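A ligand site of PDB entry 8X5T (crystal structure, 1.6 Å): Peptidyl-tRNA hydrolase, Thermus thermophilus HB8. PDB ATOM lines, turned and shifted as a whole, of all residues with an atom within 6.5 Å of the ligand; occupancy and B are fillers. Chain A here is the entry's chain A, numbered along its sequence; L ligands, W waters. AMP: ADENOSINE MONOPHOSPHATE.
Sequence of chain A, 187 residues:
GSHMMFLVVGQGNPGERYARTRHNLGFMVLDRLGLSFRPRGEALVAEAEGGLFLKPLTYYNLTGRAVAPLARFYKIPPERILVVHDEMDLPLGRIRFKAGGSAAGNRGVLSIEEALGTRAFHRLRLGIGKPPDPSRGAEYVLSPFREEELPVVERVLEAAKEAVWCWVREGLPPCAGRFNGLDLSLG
A nitrogen (N6) of the ligand sits at hydrogen-bond distance from the side-chain carboxylate (OE2) of Glu 87 (2.8 Å).
A nitrogen (N6) of the ligand sits at hydrogen-bond distance from the backbone carbonyl oxygen of Ala 104, at 2.9 Å.
The backbone NH (N) of Met 88 lies within hydrogen-bond range of a nitrogen (N1) of the ligand (3.0 Å).
The backbone NH (N) of Arg 107 lies within hydrogen-bond range of an oxygen (O2') of the ligand (3.3 Å).
The side-chain carboxylate (OE2) of Glu 87 sits at hydrogen-bond distance from the backbone NH (N) of Asp 89 (3.0 Å).
N of Ile 128 sits at hydrogen-bond distance from O of Glu 87.
The side-chain amide nitrogen (ND2) of Asn 106 lies within hydrogen-bond range of the backbone carbonyl oxygen (O) of Asp 86 (3.1 Å).
OH of Tyr 60 lies within hydrogen-bond range of ND2 of Asn 106 (2.9 Å).
N of Gly 108 lies within hydrogen-bond range of OD1 of Asn 106, 2.9 Å away.
OD2 of Asp 86 sits at hydrogen-bond distance from ND1 of His 23, at 2.7 Å.
O of Val 141 is in hydrogen-bond range of N of His 23 (2.9 Å).
The side-chain hydroxyl of Tyr 60 sits at hydrogen-bond distance from the side-chain carboxylate of Asp 86, 2.6 Å away.
The backbone carbonyl oxygen (O) of Gly 105 sits close to a nitrogen (N7) of the ligand.
Merely in contact with the ligand: His 23 (3.4 Å), Asp 86 (3.6 Å), Asn 106 (3.3 Å), Pro 134 (3.9 Å), Gly 137 (3.9 Å) and Ala 138 (3.8 Å).
Within 4 Å of the ligand: His 23, Asp 86, Glu 87, Met 88, Ala 104, Gly 105, Asn 106, Arg 107, Pro 134, Gly 137 and Ala 138.
Water W3 lies within hydrogen-bond range of O1P of the ligand (2.5 Å) and O of Gly 105 (2.6 Å).
Water W8 bridges an oxygen (O3') of the ligand and the side-chain amide nitrogen of Asn 61.
Water W5 lies within hydrogen-bond range of N7 of the ligand (2.7 Å) and O of Ala 104 (2.9 Å).
Water W7 lies within hydrogen-bond range of the backbone carbonyl oxygen (O) of Pro 134 (2.6 Å) and an oxygen (O3P) of the ligand (2.9 Å).
Water W1 bridges an oxygen (O3') of the ligand (2.9 Å) and the backbone carbonyl oxygen (O) of Ala 138 (3.4 Å).
Water W6 bridges O of Pro 134 (2.8 Å) and O3P of the ligand (3.1 Å).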
ATOM      1  N   HIS A  23     -26.117  15.523   1.584  1.00  0.00           N
ATOM      2  CA  HIS A  23     -27.126  14.714   0.884  1.00  0.00           C
ATOM      3  C   HIS A  23     -27.455  15.237  -0.507  1.00  0.00           C
ATOM      4  O   HIS A  23     -28.225  14.577  -1.250  1.00  0.00           O
ATOM      5  CB  HIS A  23     -28.416  14.570   1.759  1.00  0.00           C
ATOM      6  CG  HIS A  23     -28.837  13.179   2.099  1.00  0.00           C
ATOM      7  ND1 HIS A  23     -28.022  12.066   2.175  1.00  0.00           N
ATOM      8  CD2 HIS A  23     -30.042  12.767   2.507  1.00  0.00           C
ATOM      9  CE1 HIS A  23     -28.736  11.008   2.617  1.00  0.00           C
ATOM     10  NE2 HIS A  23     -29.978  11.423   2.795  1.00  0.00           N
ATOM     11  N   TYR A  60     -35.523  13.185  -0.958  1.00  0.00           N
ATOM     12  CA  TYR A  60     -34.443  12.215  -1.157  1.00  0.00           C
ATOM     13  C   TYR A  60     -34.968  10.779  -1.047  1.00  0.00           C
ATOM     14  O   TYR A  60     -34.558   9.900  -1.849  1.00  0.00           O
ATOM     15  CB  TYR A  60     -33.408  12.469  -0.055  1.00  0.00           C
ATOM     16  CG  TYR A  60     -32.060  11.774  -0.261  1.00  0.00           C
ATOM     17  CD1 TYR A  60     -31.844  10.448   0.072  1.00  0.00           C
ATOM     18  CD2 TYR A  60     -30.963  12.496  -0.716  1.00  0.00           C
ATOM     19  CE1 TYR A  60     -30.582   9.865  -0.084  1.00  0.00           C
ATOM     20  CE2 TYR A  60     -29.739  11.915  -0.860  1.00  0.00           C
ATOM     21  CZ  TYR A  60     -29.519  10.630  -0.561  1.00  0.00           C
ATOM     22  OH  TYR A  60     -28.302   9.990  -0.657  1.00  0.00           O
ATOM     23  N   ASN A  61     -35.861  10.516  -0.077  1.00  0.00           N
ATOM     24  CA  ASN A  61     -36.274   9.129   0.232  1.00  0.00           C
ATOM     25  C   ASN A  61     -37.483   8.723  -0.578  1.00  0.00           C
ATOM     26  O   ASN A  61     -38.001   7.604  -0.305  1.00  0.00           O
ATOM     27  CB  ASN A  61     -36.605   9.059   1.721  1.00  0.00           C
ATOM     28  CG  ASN A  61     -35.413   9.297   2.587  1.00  0.00           C
ATOM     29  OD1 ASN A  61     -34.276   9.241   2.104  1.00  0.00           O
ATOM     30  ND2 ASN A  61     -35.646   9.440   3.921  1.00  0.00           N
ATOM     31  N   HIS A  85     -24.963   9.428  -5.816  1.00  0.00           N
ATOM     32  CA  HIS A  85     -25.393   9.736  -4.416  1.00  0.00           C
ATOM     33  C   HIS A  85     -24.220   9.799  -3.498  1.00  0.00           C
ATOM     34  O   HIS A  85     -23.227   9.161  -3.686  1.00  0.00           O
ATOM     35  CB  HIS A  85     -26.395   8.667  -3.969  1.00  0.00           C
ATOM     36  CG  HIS A  85     -25.882   7.278  -3.807  1.00  0.00           C
ATOM     37  ND1 HIS A  85     -25.305   6.832  -2.646  1.00  0.00           N
ATOM     38  CD2 HIS A  85     -25.788   6.223  -4.672  1.00  0.00           C
ATOM     39  CE1 HIS A  85     -24.889   5.577  -2.787  1.00  0.00           C
ATOM     40  NE2 HIS A  85     -25.194   5.196  -4.014  1.00  0.00           N
ATOM     41  N   ASP A  86     -24.445  10.541  -2.429  1.00  0.00           N
ATOM     42  CA  ASP A  86     -23.567  10.506  -1.303  1.00  0.00           C
ATOM     43  C   ASP A  86     -23.652   9.196  -0.541  1.00  0.00           C
ATOM     44  O   ASP A  86     -24.712   8.582  -0.426  1.00  0.00           O
ATOM     45  CB  ASP A  86     -23.887  11.658  -0.340  1.00  0.00           C
ATOM     46  CG  ASP A  86     -25.326  11.637   0.145  1.00  0.00           C
ATOM     47  OD1 ASP A  86     -26.282  11.673  -0.649  1.00  0.00           O
ATOM     48  OD2 ASP A  86     -25.520  11.601   1.403  1.00  0.00           O
ATOM     49  N   GLU A  87     -22.479   8.778  -0.002  1.00  0.00           N
ATOM     50  CA  GLU A  87     -22.324   7.441   0.656  1.00  0.00           C
ATOM     51  C   GLU A  87     -21.579   7.587   1.937  1.00  0.00           C
ATOM     52  O   GLU A  87     -20.394   7.856   1.987  1.00  0.00           O
ATOM     53  CB  GLU A  87     -21.551   6.593  -0.367  1.00  0.00           C
ATOM     54  CG  GLU A  87     -21.194   5.215   0.143  1.00  0.00           C
ATOM     55  CD  GLU A  87     -22.427   4.499   0.566  1.00  0.00           C
ATOM     56  OE1 GLU A  87     -23.169   3.897  -0.315  1.00  0.00           O
ATOM     57  OE2 GLU A  87     -22.792   4.453   1.772  1.00  0.00           O
ATOM     58  N   MET A  88     -22.327   7.369   3.036  1.00  0.00           N
ATOM     59  CA  MET A  88     -21.689   7.422   4.345  1.00  0.00           C
ATOM     60  C   MET A  88     -20.701   6.279   4.565  1.00  0.00           C
ATOM     61  O   MET A  88     -19.831   6.345   5.426  1.00  0.00           O
ATOM     62  CB  MET A  88     -22.742   7.481   5.527  1.00  0.00           C
ATOM     63  CG  MET A  88     -23.402   8.789   5.685  1.00  0.00           C
ATOM     64  SD  MET A  88     -24.006   9.195   7.390  1.00  0.00           S
ATOM     65  CE  MET A  88     -25.414   8.166   7.207  1.00  0.00           C
ATOM     66  N   ASP A  89     -20.845   5.165   3.895  1.00  0.00           N
ATOM     67  CA  ASP A  89     -19.952   4.033   4.074  1.00  0.00           C
ATOM     68  C   ASP A  89     -18.685   4.106   3.320  1.00  0.00           C
ATOM     69  O   ASP A  89     -17.875   3.150   3.345  1.00  0.00           O
ATOM     70  CB  ASP A  89     -20.741   2.763   3.601  1.00  0.00           C
ATOM     71  CG  ASP A  89     -21.330   2.058   4.683  1.00  0.00           C
ATOM     72  OD1 ASP A  89     -21.631   2.705   5.791  1.00  0.00           O
ATOM     73  OD2 ASP A  89     -21.287   0.814   4.375  1.00  0.00           O
ATOM     74  N   ALA A 103     -28.257  -1.195  -0.179  1.00  0.00           N
ATOM     75  CA  ALA A 103     -28.310   0.254  -0.067  1.00  0.00           C
ATOM     76  C   ALA A 103     -27.445   0.768   1.086  1.00  0.00           C
ATOM     77  O   ALA A 103     -27.287   2.011   1.154  1.00  0.00           O
ATOM     78  CB  ALA A 103     -29.714   0.718   0.137  1.00  0.00           C
ATOM     79  N   ALA A 104     -26.945  -0.065   1.943  1.00  0.00           N
ATOM     80  CA  ALA A 104     -26.146   0.386   3.072  1.00  0.00           C
ATOM     81  C   ALA A 104     -26.865   1.423   3.960  1.00  0.00           C
ATOM     82  O   ALA A 104     -26.219   2.262   4.560  1.00  0.00           O
ATOM     83  CB  ALA A 104     -24.751   0.853   2.604  1.00  0.00           C
ATOM     84  N   GLY A 105     -28.167   1.314   4.054  1.00  0.00           N
ATOM     85  CA  GLY A 105     -28.997   2.218   4.811  1.00  0.00           C
ATOM     86  C   GLY A 105     -29.394   3.506   4.183  1.00  0.00           C
ATOM     87  O   GLY A 105     -30.190   4.272   4.750  1.00  0.00           O
ATOM     88  N   ASN A 106     -28.890   3.749   2.960  1.00  0.00           N
ATOM     89  CA  ASN A 106     -29.254   4.982   2.268  1.00  0.00           C
ATOM     90  C   ASN A 106     -30.681   4.891   1.813  1.00  0.00           C
ATOM     91  O   ASN A 106     -31.005   4.070   0.927  1.00  0.00           O
ATOM     92  CB  ASN A 106     -28.263   5.222   1.102  1.00  0.00           C
ATOM     93  CG  ASN A 106     -28.525   6.442   0.323  1.00  0.00           C
ATOM     94  OD1 ASN A 106     -29.653   6.687  -0.049  1.00  0.00           O
ATOM     95  ND2 ASN A 106     -27.514   7.265   0.129  1.00  0.00           N
ATOM     96  N   ARG A 107     -31.540   5.712   2.353  1.00  0.00           N
ATOM     97  CA  ARG A 107     -32.978   5.569   2.189  1.00  0.00           C
ATOM     98  C   ARG A 107     -33.392   6.032   0.775  1.00  0.00           C
ATOM     99  O   ARG A 107     -34.495   5.686   0.273  1.00  0.00           O
ATOM    100  CB  ARG A 107     -33.770   6.316   3.213  1.00  0.00           C
ATOM    101  CG  ARG A 107     -33.606   5.528   4.504  1.00  0.00           C
ATOM    102  CD  ARG A 107     -34.390   6.065   5.607  1.00  0.00           C
ATOM    103  NE  ARG A 107     -35.773   6.113   5.114  1.00  0.00           N
ATOM    104  CZ  ARG A 107     -36.850   6.337   5.861  1.00  0.00           C
ATOM    105  NH1 ARG A 107     -36.761   6.211   7.151  1.00  0.00           N
ATOM    106  NH2 ARG A 107     -38.029   6.548   5.254  1.00  0.00           N
ATOM    107  N   GLY A 108     -32.552   6.816   0.091  1.00  0.00           N
ATOM    108  CA  GLY A 108     -32.863   7.166  -1.292  1.00  0.00           C
ATOM    109  C   GLY A 108     -32.570   6.047  -2.283  1.00  0.00           C
ATOM    110  O   GLY A 108     -33.374   5.764  -3.184  1.00  0.00           O
ATOM    111  N   ILE A 128     -18.830  10.368   1.868  1.00  0.00           N
ATOM    112  CA  ILE A 128     -18.911  11.540   2.729  1.00  0.00           C
ATOM    113  C   ILE A 128     -18.511  11.208   4.146  1.00  0.00           C
ATOM    114  O   ILE A 128     -18.594  12.120   4.990  1.00  0.00           O
ATOM    115  CB  ILE A 128     -20.349  12.178   2.675  1.00  0.00           C
ATOM    116  CG1 ILE A 128     -21.414  11.213   3.111  1.00  0.00           C
ATOM    117  CG2 ILE A 128     -20.641  12.756   1.337  1.00  0.00           C
ATOM    118  CD1 ILE A 128     -22.723  11.849   3.513  1.00  0.00           C
ATOM    119  N   PRO A 134     -23.887   6.903  15.123  1.00  0.00           N
ATOM    120  CA  PRO A 134     -24.857   6.715  14.126  1.00  0.00           C
ATOM    121  C   PRO A 134     -26.206   7.327  14.377  1.00  0.00           C
ATOM    122  O   PRO A 134     -26.978   7.635  13.471  1.00  0.00           O
ATOM    123  CB  PRO A 134     -25.009   5.172  13.984  1.00  0.00           C
ATOM    124  CG  PRO A 134     -24.308   4.707  15.100  1.00  0.00           C
ATOM    125  CD  PRO A 134     -23.324   5.591  15.613  1.00  0.00           C
ATOM    126  N   SER A 135     -26.457   7.626  15.648  1.00  0.00           N
ATOM    127  CA  SER A 135     -27.711   8.266  15.973  1.00  0.00           C
ATOM    128  C   SER A 135     -27.813   9.721  15.608  1.00  0.00           C
ATOM    129  O   SER A 135     -28.877  10.339  15.739  1.00  0.00           O
ATOM    130  CB  SER A 135     -27.933   8.195  17.519  1.00  0.00           C
ATOM    131  OG  SER A 135     -28.199   6.829  17.828  1.00  0.00           O
ATOM    132  N   ARG A 136     -26.762  10.314  15.048  1.00  0.00           N
ATOM    133  CA  ARG A 136     -26.912  11.593  14.450  1.00  0.00           C
ATOM    134  C   ARG A 136     -26.570  11.616  12.958  1.00  0.00           C
ATOM    135  O   ARG A 136     -26.187  12.670  12.397  1.00  0.00           O
ATOM    136  CB  ARG A 136     -26.181  12.589  15.172  1.00  0.00           C
ATOM    137  CG  ARG A 136     -24.763  12.473  15.433  1.00  0.00           C
ATOM    138  CD  ARG A 136     -24.320  13.346  16.680  1.00  0.00           C
ATOM    139  NE  ARG A 136     -22.876  13.381  16.910  1.00  0.00           N
ATOM    140  CZ  ARG A 136     -21.929  14.071  16.243  1.00  0.00           C
ATOM    141  NH1 ARG A 136     -22.158  14.555  15.002  1.00  0.00           N
ATOM    142  NH2 ARG A 136     -20.634  14.045  16.735  1.00  0.00           N
ATOM    143  N   GLY A 137     -26.904  10.511  12.314  1.00  0.00           N
ATOM    144  CA  GLY A 137     -26.777  10.411  10.867  1.00  0.00           C
ATOM    145  C   GLY A 137     -27.679  11.343  10.098  1.00  0.00           C
ATOM    146  O   GLY A 137     -27.258  11.948   9.063  1.00  0.00           O
ATOM    147  N   ALA A 138     -28.918  11.590  10.515  1.00  0.00           N
ATOM    148  CA  ALA A 138     -29.816  12.425   9.773  1.00  0.00           C
ATOM    149  C   ALA A 138     -29.275  13.863   9.801  1.00  0.00           C
ATOM    150  O   ALA A 138     -29.248  14.565   8.749  1.00  0.00           O
ATOM    151  CB  ALA A 138     -31.194  12.439  10.380  1.00  0.00           C
ATOM    152  N   GLU A 139     -28.775  14.350  10.938  1.00  0.00           N
ATOM    153  CA  GLU A 139     -28.231  15.667  11.037  1.00  0.00           C
ATOM    154  C   GLU A 139     -26.947  15.735  10.155  1.00  0.00           C
ATOM    155  O   GLU A 139     -26.757  16.788   9.514  1.00  0.00           O
ATOM    156  CB  GLU A 139     -27.825  15.956  12.533  1.00  0.00           C
ATOM    157  CG  GLU A 139     -29.027  16.131  13.446  1.00  0.00           C
ATOM    158  CD  GLU A 139     -29.559  14.902  13.989  1.00  0.00           C
ATOM    159  OE1 GLU A 139     -29.225  13.741  13.672  1.00  0.00           O
ATOM    160  OE2 GLU A 139     -30.479  15.068  14.979  1.00  0.00           O
ATOM    161  N   VAL A 141     -26.072  14.135   7.394  1.00  0.00           N
ATOM    162  CA  VAL A 141     -26.335  14.249   5.927  1.00  0.00           C
ATOM    163  C   VAL A 141     -26.987  15.477   5.527  1.00  0.00           C
ATOM    164  O   VAL A 141     -26.924  15.997   4.364  1.00  0.00           O
ATOM    165  CB  VAL A 141     -26.976  12.967   5.322  1.00  0.00           C
ATOM    166  CG1 VAL A 141     -26.150  11.770   5.568  1.00  0.00           C
ATOM    167  CG2 VAL A 141     -28.439  12.843   5.773  1.00  0.00           C
ATOM    168  N   LEU A 142     -27.799  16.061   6.473  1.00  0.00           N
ATOM    169  CA  LEU A 142     -28.523  17.331   6.176  1.00  0.00           C
ATOM    170  C   LEU A 142     -27.741  18.591   6.609  1.00  0.00           C
ATOM    171  O   LEU A 142     -28.319  19.655   6.725  1.00  0.00           O
ATOM    172  CB  LEU A 142     -29.975  17.301   6.748  1.00  0.00           C
ATOM    173  CG  LEU A 142     -30.815  16.199   6.162  1.00  0.00           C
ATOM    174  CD1 LEU A 142     -32.221  16.198   6.829  1.00  0.00           C
ATOM    175  CD2 LEU A 142     -30.974  16.335   4.672  1.00  0.00           C
HETATM  176  P   AMP L   1     -30.578   5.826   9.917  1.00  0.00           P
HETATM  177  O1P AMP L   1     -30.756   4.486   9.248  1.00  0.00           O
HETATM  178  O2P AMP L   1     -32.034   5.956   9.755  1.00  0.00           O
HETATM  179  O3P AMP L   1     -29.364   5.990  10.845  1.00  0.00           O
HETATM  180  O5' AMP L   1     -30.190   6.836   8.797  1.00  0.00           O
HETATM  181  C5' AMP L   1     -29.820   8.156   9.182  1.00  0.00           C
HETATM  182  C4' AMP L   1     -29.972   8.976   7.955  1.00  0.00           C
HETATM  183  O4' AMP L   1     -28.818   8.693   7.175  1.00  0.00           O
HETATM  184  C3' AMP L   1     -31.146   8.834   7.073  1.00  0.00           C
HETATM  185  O3' AMP L   1     -31.562  10.071   6.463  1.00  0.00           O
HETATM  186  C2' AMP L   1     -30.591   7.856   6.069  1.00  0.00           C
HETATM  187  O2' AMP L   1     -31.224   7.875   4.776  1.00  0.00           O
HETATM  188  C1' AMP L   1     -29.160   8.341   5.828  1.00  0.00           C
HETATM  189  N9  AMP L   1     -28.272   7.294   5.495  1.00  0.00           N
HETATM  190  C8  AMP L   1     -28.046   6.072   6.124  1.00  0.00           C
HETATM  191  N7  AMP L   1     -27.151   5.271   5.596  1.00  0.00           N
HETATM  192  C5  AMP L   1     -26.641   6.072   4.566  1.00  0.00           C
HETATM  193  C6  AMP L   1     -25.584   5.775   3.665  1.00  0.00           C
HETATM  194  N6  AMP L   1     -24.906   4.631   3.563  1.00  0.00           N
HETATM  195  N1  AMP L   1     -25.268   6.882   2.849  1.00  0.00           N
HETATM  196  C2  AMP L   1     -25.984   8.039   2.946  1.00  0.00           C
HETATM  197  N3  AMP L   1     -27.015   8.339   3.701  1.00  0.00           N
HETATM  198  C4  AMP L   1     -27.272   7.316   4.529  1.00  0.00           C
HETATM  199  O   HOH W   1     -31.625  12.883   6.971  1.00  0.00           O
HETATM  200  O   HOH W   2     -28.367   3.190   8.658  1.00  0.00           O
HETATM  201  O   HOH W   3     -31.420   3.750   7.003  1.00  0.00           O
HETATM  202  O   HOH W   4     -32.213  10.110   3.571  1.00  0.00           O
HETATM  203  O   HOH W   5     -26.053   3.380   7.208  1.00  0.00           O
HETATM  204  O   HOH W   6     -26.463   7.025  10.798  1.00  0.00           O
HETATM  205  O   HOH W   7     -29.439   8.095  12.768  1.00  0.00           O
HETATM  206  O   HOH W   8     -34.276   9.993   6.512  1.00  0.00           O
